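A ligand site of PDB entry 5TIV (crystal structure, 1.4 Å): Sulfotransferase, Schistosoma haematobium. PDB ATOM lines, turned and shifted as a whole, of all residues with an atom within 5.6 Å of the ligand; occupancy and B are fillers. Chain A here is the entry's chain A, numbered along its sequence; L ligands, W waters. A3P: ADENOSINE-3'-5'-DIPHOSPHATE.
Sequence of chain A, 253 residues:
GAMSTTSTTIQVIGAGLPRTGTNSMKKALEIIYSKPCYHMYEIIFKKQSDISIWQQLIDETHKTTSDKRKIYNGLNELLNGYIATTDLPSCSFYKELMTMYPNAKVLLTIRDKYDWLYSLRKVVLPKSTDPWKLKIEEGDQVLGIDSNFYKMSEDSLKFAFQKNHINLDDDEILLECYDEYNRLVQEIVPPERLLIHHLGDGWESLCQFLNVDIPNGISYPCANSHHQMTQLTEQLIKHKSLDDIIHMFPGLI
The side-chain hydroxyl of Ser 119 sits at hydrogen-bond distance from an oxygen (O2P) of the ligand, 2.5 Å away.
N of Thr 22 is in hydrogen-bond range of O4P of the ligand (2.7 Å).
The side-chain hydroxyl of Thr 22 is in hydrogen-bond range of an oxygen (O4P) of the ligand (2.7 Å).
An oxygen (O4P) of the ligand is in hydrogen-bond range of the backbone NH (N) of Arg 19 (3.0 Å).
The guanidinium group of Arg 19 is in salt-bridge range of an oxygen (O6P) of the ligand (2.8 Å).
OG of Ser 24 lies within hydrogen-bond range of N7 of the ligand (2.8 Å).
The guanidinium group of Arg 111 lies within salt-bridge range of an oxygen (O1P) of the ligand (2.9 Å).
The backbone NH of Asn 23 sits at hydrogen-bond distance from an oxygen (O5P) of the ligand (2.9 Å).
The backbone carbonyl oxygen of Pro 221 is in hydrogen-bond range of a nitrogen (N6) of the ligand (3.0 Å).
The side-chain amide nitrogen (ND2) of Asn 224 lies within hydrogen-bond range of an oxygen (O5P) of the ligand.
N of Gly 21 sits at hydrogen-bond distance from O5' of the ligand, 3.0 Å away.
N of His 226 sits at hydrogen-bond distance from O2P of the ligand, 3.0 Å away.
An oxygen (O4P) of the ligand sits at hydrogen-bond distance from the backbone NH (N) of Thr 20.
The guanidinium group (NE) of Arg 19 is in hydrogen-bond range of the side-chain hydroxyl (OG) of Ser 119, 2.8 Å away.
A ring nitrogen (NE2) of His 39 lies within hydrogen-bond range of the side-chain hydroxyl (OG1) of Thr 22 (3.0 Å).
O of Arg 19 sits at hydrogen-bond distance from NH1 of Arg 111 (2.9 Å).
NH2 of Arg 19 lies within hydrogen-bond range of O of Asn 224 (2.8 Å).
The side-chain hydroxyl of Ser 24 is in hydrogen-bond range of the backbone carbonyl oxygen of Pro 221 (3.2 Å).
A ring nitrogen (NE2) of His 39 sits at hydrogen-bond distance from the backbone NH (N) of Asn 23 (3.4 Å).
OG1 of Thr 20 sits at hydrogen-bond distance from O of Leu 17 (2.7 Å).
Residues that only touch the ligand: Leu 199 (3.4 Å), Tyr 220 (3.8 Å), Cys 222 (3.7 Å), Ala 223 (3.5 Å) and Ser 225 (3.4 Å).
Hydrophobic or aromatic side chains within 4 Å of the ligand: Leu 199, Tyr 220 and His 226.
Of the 24 residues printed, 16 come within 4 Å of the ligand.
Water W5 lies within hydrogen-bond range of O5P of the ligand (2.6 Å), N of Ser 24 (3.0 Å), O of Ala 223 (3.0 Å) and N of Asn 23 (3.5 Å).
Water W2 lies within hydrogen-bond range of an oxygen (O2') of the ligand (2.7 Å) and the backbone carbonyl oxygen of Cys 222 (2.9 Å).
Water W6 lies within hydrogen-bond range of O6P of the ligand (2.8 Å), OD1 of Asp 87 (3.2 Å) and N of Arg 19 (3.4 Å).
Water W3 bridges O1P of the ligand and O of Asp 115.
Water W1 lies within hydrogen-bond range of an oxygen (O1P) of the ligand (2.9 Å) and the guanidinium group (NH2) of Arg 111 (3.4 Å).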
ATOM      1  N   LEU A  17     -20.750 -19.530 -13.289  1.00  0.00           N
ATOM      2  CA  LEU A  17     -21.538 -20.466 -12.516  1.00  0.00           C
ATOM      3  C   LEU A  17     -23.001 -20.008 -12.372  1.00  0.00           C
ATOM      4  O   LEU A  17     -23.332 -18.830 -12.568  1.00  0.00           O
ATOM      5  CB  LEU A  17     -20.881 -20.617 -11.127  1.00  0.00           C
ATOM      6  CG  LEU A  17     -19.528 -21.334 -11.153  1.00  0.00           C
ATOM      7  CD1 LEU A  17     -18.758 -21.137  -9.836  1.00  0.00           C
ATOM      8  CD2 LEU A  17     -19.716 -22.788 -11.440  1.00  0.00           C
ATOM      9  N   PRO A  18     -23.879 -20.915 -11.987  1.00  0.00           N
ATOM     10  CA  PRO A  18     -25.258 -20.515 -11.701  1.00  0.00           C
ATOM     11  C   PRO A  18     -25.295 -19.390 -10.669  1.00  0.00           C
ATOM     12  O   PRO A  18     -24.471 -19.344  -9.756  1.00  0.00           O
ATOM     13  CB  PRO A  18     -25.923 -21.799 -11.181  1.00  0.00           C
ATOM     14  CG  PRO A  18     -24.813 -22.718 -10.848  1.00  0.00           C
ATOM     15  CD  PRO A  18     -23.656 -22.353 -11.738  1.00  0.00           C
ATOM     16  N   ARG A  19     -26.298 -18.514 -10.809  1.00  0.00           N
ATOM     17  CA  ARG A  19     -26.541 -17.393  -9.912  1.00  0.00           C
ATOM     18  C   ARG A  19     -25.494 -16.290 -10.055  1.00  0.00           C
ATOM     19  O   ARG A  19     -25.340 -15.481  -9.147  1.00  0.00           O
ATOM     20  CB  ARG A  19     -26.755 -17.818  -8.449  1.00  0.00           C
ATOM     21  CG  ARG A  19     -27.796 -18.925  -8.299  1.00  0.00           C
ATOM     22  CD  ARG A  19     -29.116 -18.684  -9.011  1.00  0.00           C
ATOM     23  NE  ARG A  19     -29.826 -17.566  -8.436  1.00  0.00           N
ATOM     24  CZ  ARG A  19     -30.939 -17.034  -8.948  1.00  0.00           C
ATOM     25  NH1 ARG A  19     -31.442 -17.480 -10.089  1.00  0.00           N
ATOM     26  NH2 ARG A  19     -31.539 -16.037  -8.316  1.00  0.00           N
ATOM     27  N   THR A  20     -24.833 -16.193 -11.213  1.00  0.00           N
ATOM     28  CA  THR A  20     -23.930 -15.085 -11.509  1.00  0.00           C
ATOM     29  C   THR A  20     -24.481 -14.175 -12.613  1.00  0.00           C
ATOM     30  O   THR A  20     -23.709 -13.430 -13.215  1.00  0.00           O
ATOM     31  CB  THR A  20     -22.521 -15.565 -11.895  1.00  0.00           C
ATOM     32  OG1 THR A  20     -22.572 -16.344 -13.092  1.00  0.00           O
ATOM     33  CG2 THR A  20     -21.878 -16.369 -10.741  1.00  0.00           C
ATOM     34  N   GLY A  21     -25.773 -14.205 -12.867  1.00  0.00           N
ATOM     35  CA  GLY A  21     -26.337 -13.393 -13.934  1.00  0.00           C
ATOM     36  C   GLY A  21     -26.388 -14.095 -15.276  1.00  0.00           C
ATOM     37  O   GLY A  21     -26.326 -13.427 -16.319  1.00  0.00           O
ATOM     38  N   THR A  22     -26.502 -15.422 -15.266  1.00  0.00           N
ATOM     39  CA  THR A  22     -26.430 -16.175 -16.512  1.00  0.00           C
ATOM     40  C   THR A  22     -27.680 -16.005 -17.353  1.00  0.00           C
ATOM     41  O   THR A  22     -27.591 -15.994 -18.596  1.00  0.00           O
ATOM     42  CB  THR A  22     -26.151 -17.653 -16.251  1.00  0.00           C
ATOM     43  OG1 THR A  22     -27.264 -18.261 -15.589  1.00  0.00           O
ATOM     44  CG2 THR A  22     -24.848 -17.860 -15.469  1.00  0.00           C
ATOM     45  N   ASN A  23     -28.852 -15.902 -16.733  1.00  0.00           N
ATOM     46  CA  ASN A  23     -30.057 -15.679 -17.517  1.00  0.00           C
ATOM     47  C   ASN A  23     -30.048 -14.306 -18.181  1.00  0.00           C
ATOM     48  O   ASN A  23     -30.420 -14.174 -19.356  1.00  0.00           O
ATOM     49  CB  ASN A  23     -31.301 -15.881 -16.661  1.00  0.00           C
ATOM     50  CG  ASN A  23     -32.537 -15.876 -17.479  1.00  0.00           C
ATOM     51  OD1 ASN A  23     -33.279 -14.905 -17.502  1.00  0.00           O
ATOM     52  ND2 ASN A  23     -32.750 -16.970 -18.196  1.00  0.00           N
ATOM     53  N   SER A  24     -29.577 -13.293 -17.469  1.00  0.00           N
ATOM     54  CA  SER A  24     -29.437 -11.978 -18.096  1.00  0.00           C
ATOM     55  C   SER A  24     -28.415 -11.983 -19.215  1.00  0.00           C
ATOM     56  O   SER A  24     -28.616 -11.322 -20.235  1.00  0.00           O
ATOM     57  CB  SER A  24     -29.059 -10.940 -17.049  1.00  0.00           C
ATOM     58  OG  SER A  24     -30.127 -10.715 -16.177  1.00  0.00           O
ATOM     59  N   HIS A  39     -29.316 -22.276 -22.081  1.00  0.00           N
ATOM     60  CA  HIS A  39     -29.373 -21.965 -20.655  1.00  0.00           C
ATOM     61  C   HIS A  39     -30.140 -23.089 -19.989  1.00  0.00           C
ATOM     62  O   HIS A  39     -30.854 -23.844 -20.645  1.00  0.00           O
ATOM     63  CB  HIS A  39     -30.119 -20.631 -20.432  1.00  0.00           C
ATOM     64  CG  HIS A  39     -30.081 -20.119 -19.029  1.00  0.00           C
ATOM     65  ND1 HIS A  39     -31.058 -20.412 -18.101  1.00  0.00           N
ATOM     66  CD2 HIS A  39     -29.203 -19.315 -18.396  1.00  0.00           C
ATOM     67  CE1 HIS A  39     -30.772 -19.825 -16.952  1.00  0.00           C
ATOM     68  NE2 HIS A  39     -29.647 -19.149 -17.099  1.00  0.00           N
ATOM     69  N   ASP A  87     -24.861 -20.852 -18.070  1.00  0.00           N
ATOM     70  CA  ASP A  87     -25.392 -21.568 -16.918  1.00  0.00           C
ATOM     71  C   ASP A  87     -24.987 -23.038 -16.890  1.00  0.00           C
ATOM     72  O   ASP A  87     -24.362 -23.551 -17.818  1.00  0.00           O
ATOM     73  CB  ASP A  87     -26.927 -21.475 -16.904  1.00  0.00           C
ATOM     74  CG  ASP A  87     -27.534 -21.618 -15.506  1.00  0.00           C
ATOM     75  OD1 ASP A  87     -26.840 -21.863 -14.494  1.00  0.00           O
ATOM     76  OD2 ASP A  87     -28.781 -21.482 -15.438  1.00  0.00           O
ATOM     77  N   ARG A 111     -19.517 -12.535  -9.412  1.00  0.00           N
ATOM     78  CA  ARG A 111     -20.040 -11.624  -8.405  1.00  0.00           C
ATOM     79  C   ARG A 111     -19.392 -11.929  -7.070  1.00  0.00           C
ATOM     80  O   ARG A 111     -18.684 -12.935  -6.902  1.00  0.00           O
ATOM     81  CB  ARG A 111     -21.562 -11.763  -8.306  1.00  0.00           C
ATOM     82  CG  ARG A 111     -21.970 -13.075  -7.676  1.00  0.00           C
ATOM     83  CD  ARG A 111     -23.459 -13.319  -7.714  1.00  0.00           C
ATOM     84  NE  ARG A 111     -24.221 -12.349  -6.950  1.00  0.00           N
ATOM     85  CZ  ARG A 111     -25.535 -12.419  -6.796  1.00  0.00           C
ATOM     86  NH1 ARG A 111     -26.229 -13.456  -7.273  1.00  0.00           N
ATOM     87  NH2 ARG A 111     -26.155 -11.477  -6.138  1.00  0.00           N
ATOM     88  N   ASP A 115     -22.699 -13.144  -1.718  1.00  0.00           N
ATOM     89  CA  ASP A 115     -23.966 -12.956  -2.392  1.00  0.00           C
ATOM     90  C   ASP A 115     -24.288 -14.147  -3.277  1.00  0.00           C
ATOM     91  O   ASP A 115     -25.439 -14.580  -3.362  1.00  0.00           O
ATOM     92  CB  ASP A 115     -23.933 -11.712  -3.278  1.00  0.00           C
ATOM     93  CG  ASP A 115     -23.819 -10.392  -2.494  1.00  0.00           C
ATOM     94  OD1 ASP A 115     -24.090 -10.345  -1.272  1.00  0.00           O
ATOM     95  OD2 ASP A 115     -23.497  -9.391  -3.157  1.00  0.00           O
ATOM     96  N   SER A 119     -27.617 -16.672  -2.935  1.00  0.00           N
ATOM     97  CA  SER A 119     -28.511 -16.883  -4.053  1.00  0.00           C
ATOM     98  C   SER A 119     -28.577 -18.355  -4.436  1.00  0.00           C
ATOM     99  O   SER A 119     -29.647 -18.883  -4.741  1.00  0.00           O
ATOM    100  CB  SER A 119     -27.970 -16.052  -5.210  1.00  0.00           C
ATOM    101  OG  SER A 119     -28.852 -16.060  -6.304  1.00  0.00           O
ATOM    102  N   VAL A 123     -32.070 -20.973  -4.532  1.00  0.00           N
ATOM    103  CA  VAL A 123     -32.640 -21.322  -5.833  1.00  0.00           C
ATOM    104  C   VAL A 123     -32.192 -22.677  -6.364  1.00  0.00           C
ATOM    105  O   VAL A 123     -33.015 -23.492  -6.779  1.00  0.00           O
ATOM    106  CB  VAL A 123     -32.355 -20.213  -6.878  1.00  0.00           C
ATOM    107  CG1 VAL A 123     -32.939 -20.566  -8.231  1.00  0.00           C
ATOM    108  CG2 VAL A 123     -32.893 -18.878  -6.386  1.00  0.00           C
ATOM    109  N   LEU A 199     -21.341  -8.609 -12.146  1.00  0.00           N
ATOM    110  CA  LEU A 199     -22.739  -8.262 -12.033  1.00  0.00           C
ATOM    111  C   LEU A 199     -22.849  -6.749 -11.965  1.00  0.00           C
ATOM    112  O   LEU A 199     -22.162  -6.103 -11.160  1.00  0.00           O
ATOM    113  CB  LEU A 199     -23.321  -8.928 -10.782  1.00  0.00           C
ATOM    114  CG  LEU A 199     -24.758  -9.395 -10.766  1.00  0.00           C
ATOM    115  CD1 LEU A 199     -25.156 -10.245 -11.984  1.00  0.00           C
ATOM    116  CD2 LEU A 199     -24.994 -10.160  -9.476  1.00  0.00           C
ATOM    117  N   GLY A 200     -23.669  -6.190 -12.852  1.00  0.00           N
ATOM    118  CA  GLY A 200     -23.839  -4.755 -12.984  1.00  0.00           C
ATOM    119  C   GLY A 200     -23.016  -4.085 -14.071  1.00  0.00           C
ATOM    120  O   GLY A 200     -23.208  -2.873 -14.294  1.00  0.00           O
ATOM    121  N   TYR A 220     -29.887  -3.367 -20.440  1.00  0.00           N
ATOM    122  CA  TYR A 220     -29.287  -4.655 -20.158  1.00  0.00           C
ATOM    123  C   TYR A 220     -30.234  -5.470 -19.273  1.00  0.00           C
ATOM    124  O   TYR A 220     -30.784  -4.934 -18.308  1.00  0.00           O
ATOM    125  CB  TYR A 220     -27.947  -4.462 -19.449  1.00  0.00           C
ATOM    126  CG  TYR A 220     -27.205  -5.754 -19.316  1.00  0.00           C
ATOM    127  CD1 TYR A 220     -26.400  -6.223 -20.348  1.00  0.00           C
ATOM    128  CD2 TYR A 220     -27.346  -6.542 -18.192  1.00  0.00           C
ATOM    129  CE1 TYR A 220     -25.752  -7.417 -20.259  1.00  0.00           C
ATOM    130  CE2 TYR A 220     -26.707  -7.744 -18.085  1.00  0.00           C
ATOM    131  CZ  TYR A 220     -25.895  -8.180 -19.115  1.00  0.00           C
ATOM    132  OH  TYR A 220     -25.257  -9.393 -19.029  1.00  0.00           O
ATOM    133  N   PRO A 221     -30.461  -6.766 -19.583  1.00  0.00           N
ATOM    134  CA  PRO A 221     -31.455  -7.545 -18.815  1.00  0.00           C
ATOM    135  C   PRO A 221     -31.113  -7.667 -17.344  1.00  0.00           C
ATOM    136  O   PRO A 221     -29.944  -7.651 -16.955  1.00  0.00           O
ATOM    137  CB  PRO A 221     -31.418  -8.921 -19.502  1.00  0.00           C
ATOM    138  CG  PRO A 221     -30.924  -8.631 -20.922  1.00  0.00           C
ATOM    139  CD  PRO A 221     -29.934  -7.508 -20.735  1.00  0.00           C
ATOM    140  N   CYS A 222     -32.164  -7.883 -16.492  1.00  0.00           N
ATOM    141  CA  CYS A 222     -31.975  -7.840 -15.039  1.00  0.00           C
ATOM    142  C   CYS A 222     -32.870  -8.801 -14.245  1.00  0.00           C
ATOM    143  O   CYS A 222     -33.174  -8.538 -13.071  1.00  0.00           O
ATOM    144  CB  CYS A 222     -32.217  -6.430 -14.491  1.00  0.00           C
ATOM    145  SG  CYS A 222     -33.903  -5.839 -14.799  1.00  0.00           S
ATOM    146  N   ALA A 223     -33.263  -9.934 -14.823  1.00  0.00           N
ATOM    147  CA  ALA A 223     -34.250 -10.807 -14.205  1.00  0.00           C
ATOM    148  C   ALA A 223     -33.587 -12.014 -13.554  1.00  0.00           C
ATOM    149  O   ALA A 223     -32.359 -12.147 -13.511  1.00  0.00           O
ATOM    150  CB  ALA A 223     -35.368 -11.224 -15.155  1.00  0.00           C
ATOM    151  N   ASN A 224     -34.437 -12.867 -13.002  1.00  0.00           N
ATOM    152  CA  ASN A 224     -34.066 -14.116 -12.341  1.00  0.00           C
ATOM    153  C   ASN A 224     -33.513 -13.901 -10.934  1.00  0.00           C
ATOM    154  O   ASN A 224     -32.749 -14.725 -10.459  1.00  0.00           O
ATOM    155  CB  ASN A 224     -33.078 -14.920 -13.197  1.00  0.00           C
ATOM    156  CG  ASN A 224     -33.255 -16.421 -13.052  1.00  0.00           C
ATOM    157  OD1 ASN A 224     -34.330 -16.932 -12.695  1.00  0.00           O
ATOM    158  ND2 ASN A 224     -32.190 -17.139 -13.319  1.00  0.00           N
ATOM    159  N   SER A 225     -33.938 -12.853 -10.244  1.00  0.00           N
ATOM    160  CA  SER A 225     -33.521 -12.633  -8.861  1.00  0.00           C
ATOM    161  C   SER A 225     -34.092 -13.722  -7.966  1.00  0.00           C
ATOM    162  O   SER A 225     -35.084 -14.361  -8.284  1.00  0.00           O
ATOM    163  CB  SER A 225     -34.035 -11.293  -8.387  1.00  0.00           C
ATOM    164  OG  SER A 225     -35.437 -11.327  -8.203  1.00  0.00           O
ATOM    165  N   HIS A 226     -33.429 -13.951  -6.822  1.00  0.00           N
ATOM    166  CA  HIS A 226     -33.970 -14.960  -5.915  1.00  0.00           C
ATOM    167  C   HIS A 226     -35.343 -14.561  -5.389  1.00  0.00           C
ATOM    168  O   HIS A 226     -36.167 -15.438  -5.125  1.00  0.00           O
ATOM    169  CB  HIS A 226     -32.988 -15.366  -4.791  1.00  0.00           C
ATOM    170  CG  HIS A 226     -32.756 -14.329  -3.734  1.00  0.00           C
ATOM    171  ND1 HIS A 226     -33.638 -14.088  -2.700  1.00  0.00           N
ATOM    172  CD2 HIS A 226     -31.661 -13.552  -3.476  1.00  0.00           C
ATOM    173  CE1 HIS A 226     -33.127 -13.174  -1.881  1.00  0.00           C
ATOM    174  NE2 HIS A 226     -31.931 -12.826  -2.343  1.00  0.00           N
ATOM    175  N   HIS A 227     -35.623 -13.261  -5.269  1.00  0.00           N
ATOM    176  CA  HIS A 227     -36.965 -12.842  -4.880  1.00  0.00           C
ATOM    177  C   HIS A 227     -37.989 -13.304  -5.888  1.00  0.00           C
ATOM    178  O   HIS A 227     -39.056 -13.811  -5.520  1.00  0.00           O
ATOM    179  CB  HIS A 227     -37.039 -11.324  -4.749  1.00  0.00           C
ATOM    180  CG  HIS A 227     -36.092 -10.781  -3.736  1.00  0.00           C
ATOM    181  ND1 HIS A 227     -36.006 -11.292  -2.457  1.00  0.00           N
ATOM    182  CD2 HIS A 227     -35.185  -9.781  -3.807  1.00  0.00           C
ATOM    183  CE1 HIS A 227     -35.079 -10.623  -1.782  1.00  0.00           C
ATOM    184  NE2 HIS A 227     -34.561  -9.703  -2.579  1.00  0.00           N
HETATM  185  P1  A3P L   1     -29.905 -12.680  -6.667  1.00  0.00           P
HETATM  186  O1P A3P L   1     -28.893 -12.269  -5.623  1.00  0.00           O
HETATM  187  O2P A3P L   1     -30.427 -14.068  -6.522  1.00  0.00           O
HETATM  188  O3P A3P L   1     -30.987 -11.674  -6.871  1.00  0.00           O
HETATM  189  P2  A3P L   1     -28.678 -16.584 -12.783  1.00  0.00           P
HETATM  190  O4P A3P L   1     -27.323 -17.051 -13.217  1.00  0.00           O
HETATM  191  O5P A3P L   1     -29.533 -15.983 -13.886  1.00  0.00           O
HETATM  192  O6P A3P L   1     -29.395 -17.622 -11.994  1.00  0.00           O
HETATM  193  O5' A3P L   1     -28.335 -15.342 -11.806  1.00  0.00           O
HETATM  194  C5' A3P L   1     -29.355 -14.619 -11.132  1.00  0.00           C
HETATM  195  C4' A3P L   1     -28.720 -13.610 -10.191  1.00  0.00           C
HETATM  196  O4' A3P L   1     -28.128 -12.539 -10.932  1.00  0.00           O
HETATM  197  C3' A3P L   1     -29.736 -12.966  -9.284  1.00  0.00           C
HETATM  198  O3' A3P L   1     -29.080 -12.666  -8.051  1.00  0.00           O
HETATM  199  C2' A3P L   1     -30.077 -11.689 -10.030  1.00  0.00           C
HETATM  200  O2' A3P L   1     -30.652 -10.680  -9.212  1.00  0.00           O
HETATM  201  C1' A3P L   1     -28.712 -11.301 -10.543  1.00  0.00           C
HETATM  202  N9  A3P L   1     -28.769 -10.396 -11.708  1.00  0.00           N
HETATM  203  C8  A3P L   1     -29.173 -10.733 -12.940  1.00  0.00           C
HETATM  204  N7  A3P L   1     -29.073  -9.678 -13.775  1.00  0.00           N
HETATM  205  C5  A3P L   1     -28.605  -8.645 -13.078  1.00  0.00           C
HETATM  206  C6  A3P L   1     -28.275  -7.235 -13.366  1.00  0.00           C
HETATM  207  N6  A3P L   1     -28.432  -6.710 -14.601  1.00  0.00           N
HETATM  208  N1  A3P L   1     -27.800  -6.491 -12.343  1.00  0.00           N
HETATM  209  C2  A3P L   1     -27.641  -7.009 -11.121  1.00  0.00           C
HETATM  210  N3  A3P L   1     -27.918  -8.269 -10.789  1.00  0.00           N
HETATM  211  C4  A3P L   1     -28.392  -9.125 -11.709  1.00  0.00           C
HETATM  212  O   HOH W   1     -28.828  -9.412  -5.532  1.00  0.00           O
HETATM  213  O   HOH W   2     -31.884  -8.597 -10.420  1.00  0.00           O
HETATM  214  O   HOH W   3     -27.812 -13.043  -3.147  1.00  0.00           O
HETATM  215  O   HOH W   4     -27.502  -3.747 -12.364  1.00  0.00           O
HETATM  216  O   HOH W   5     -29.788 -13.455 -14.468  1.00  0.00           O
HETATM  217  O   HOH W   6     -28.687 -20.275 -12.487  1.00  0.00           O
HETATM  218  O   HOH W   7     -27.076  -3.911 -15.609  1.00  0.00           O
HETATM  219  O   HOH W   8     -27.951  -8.142  -7.857  1.00  0.00           O
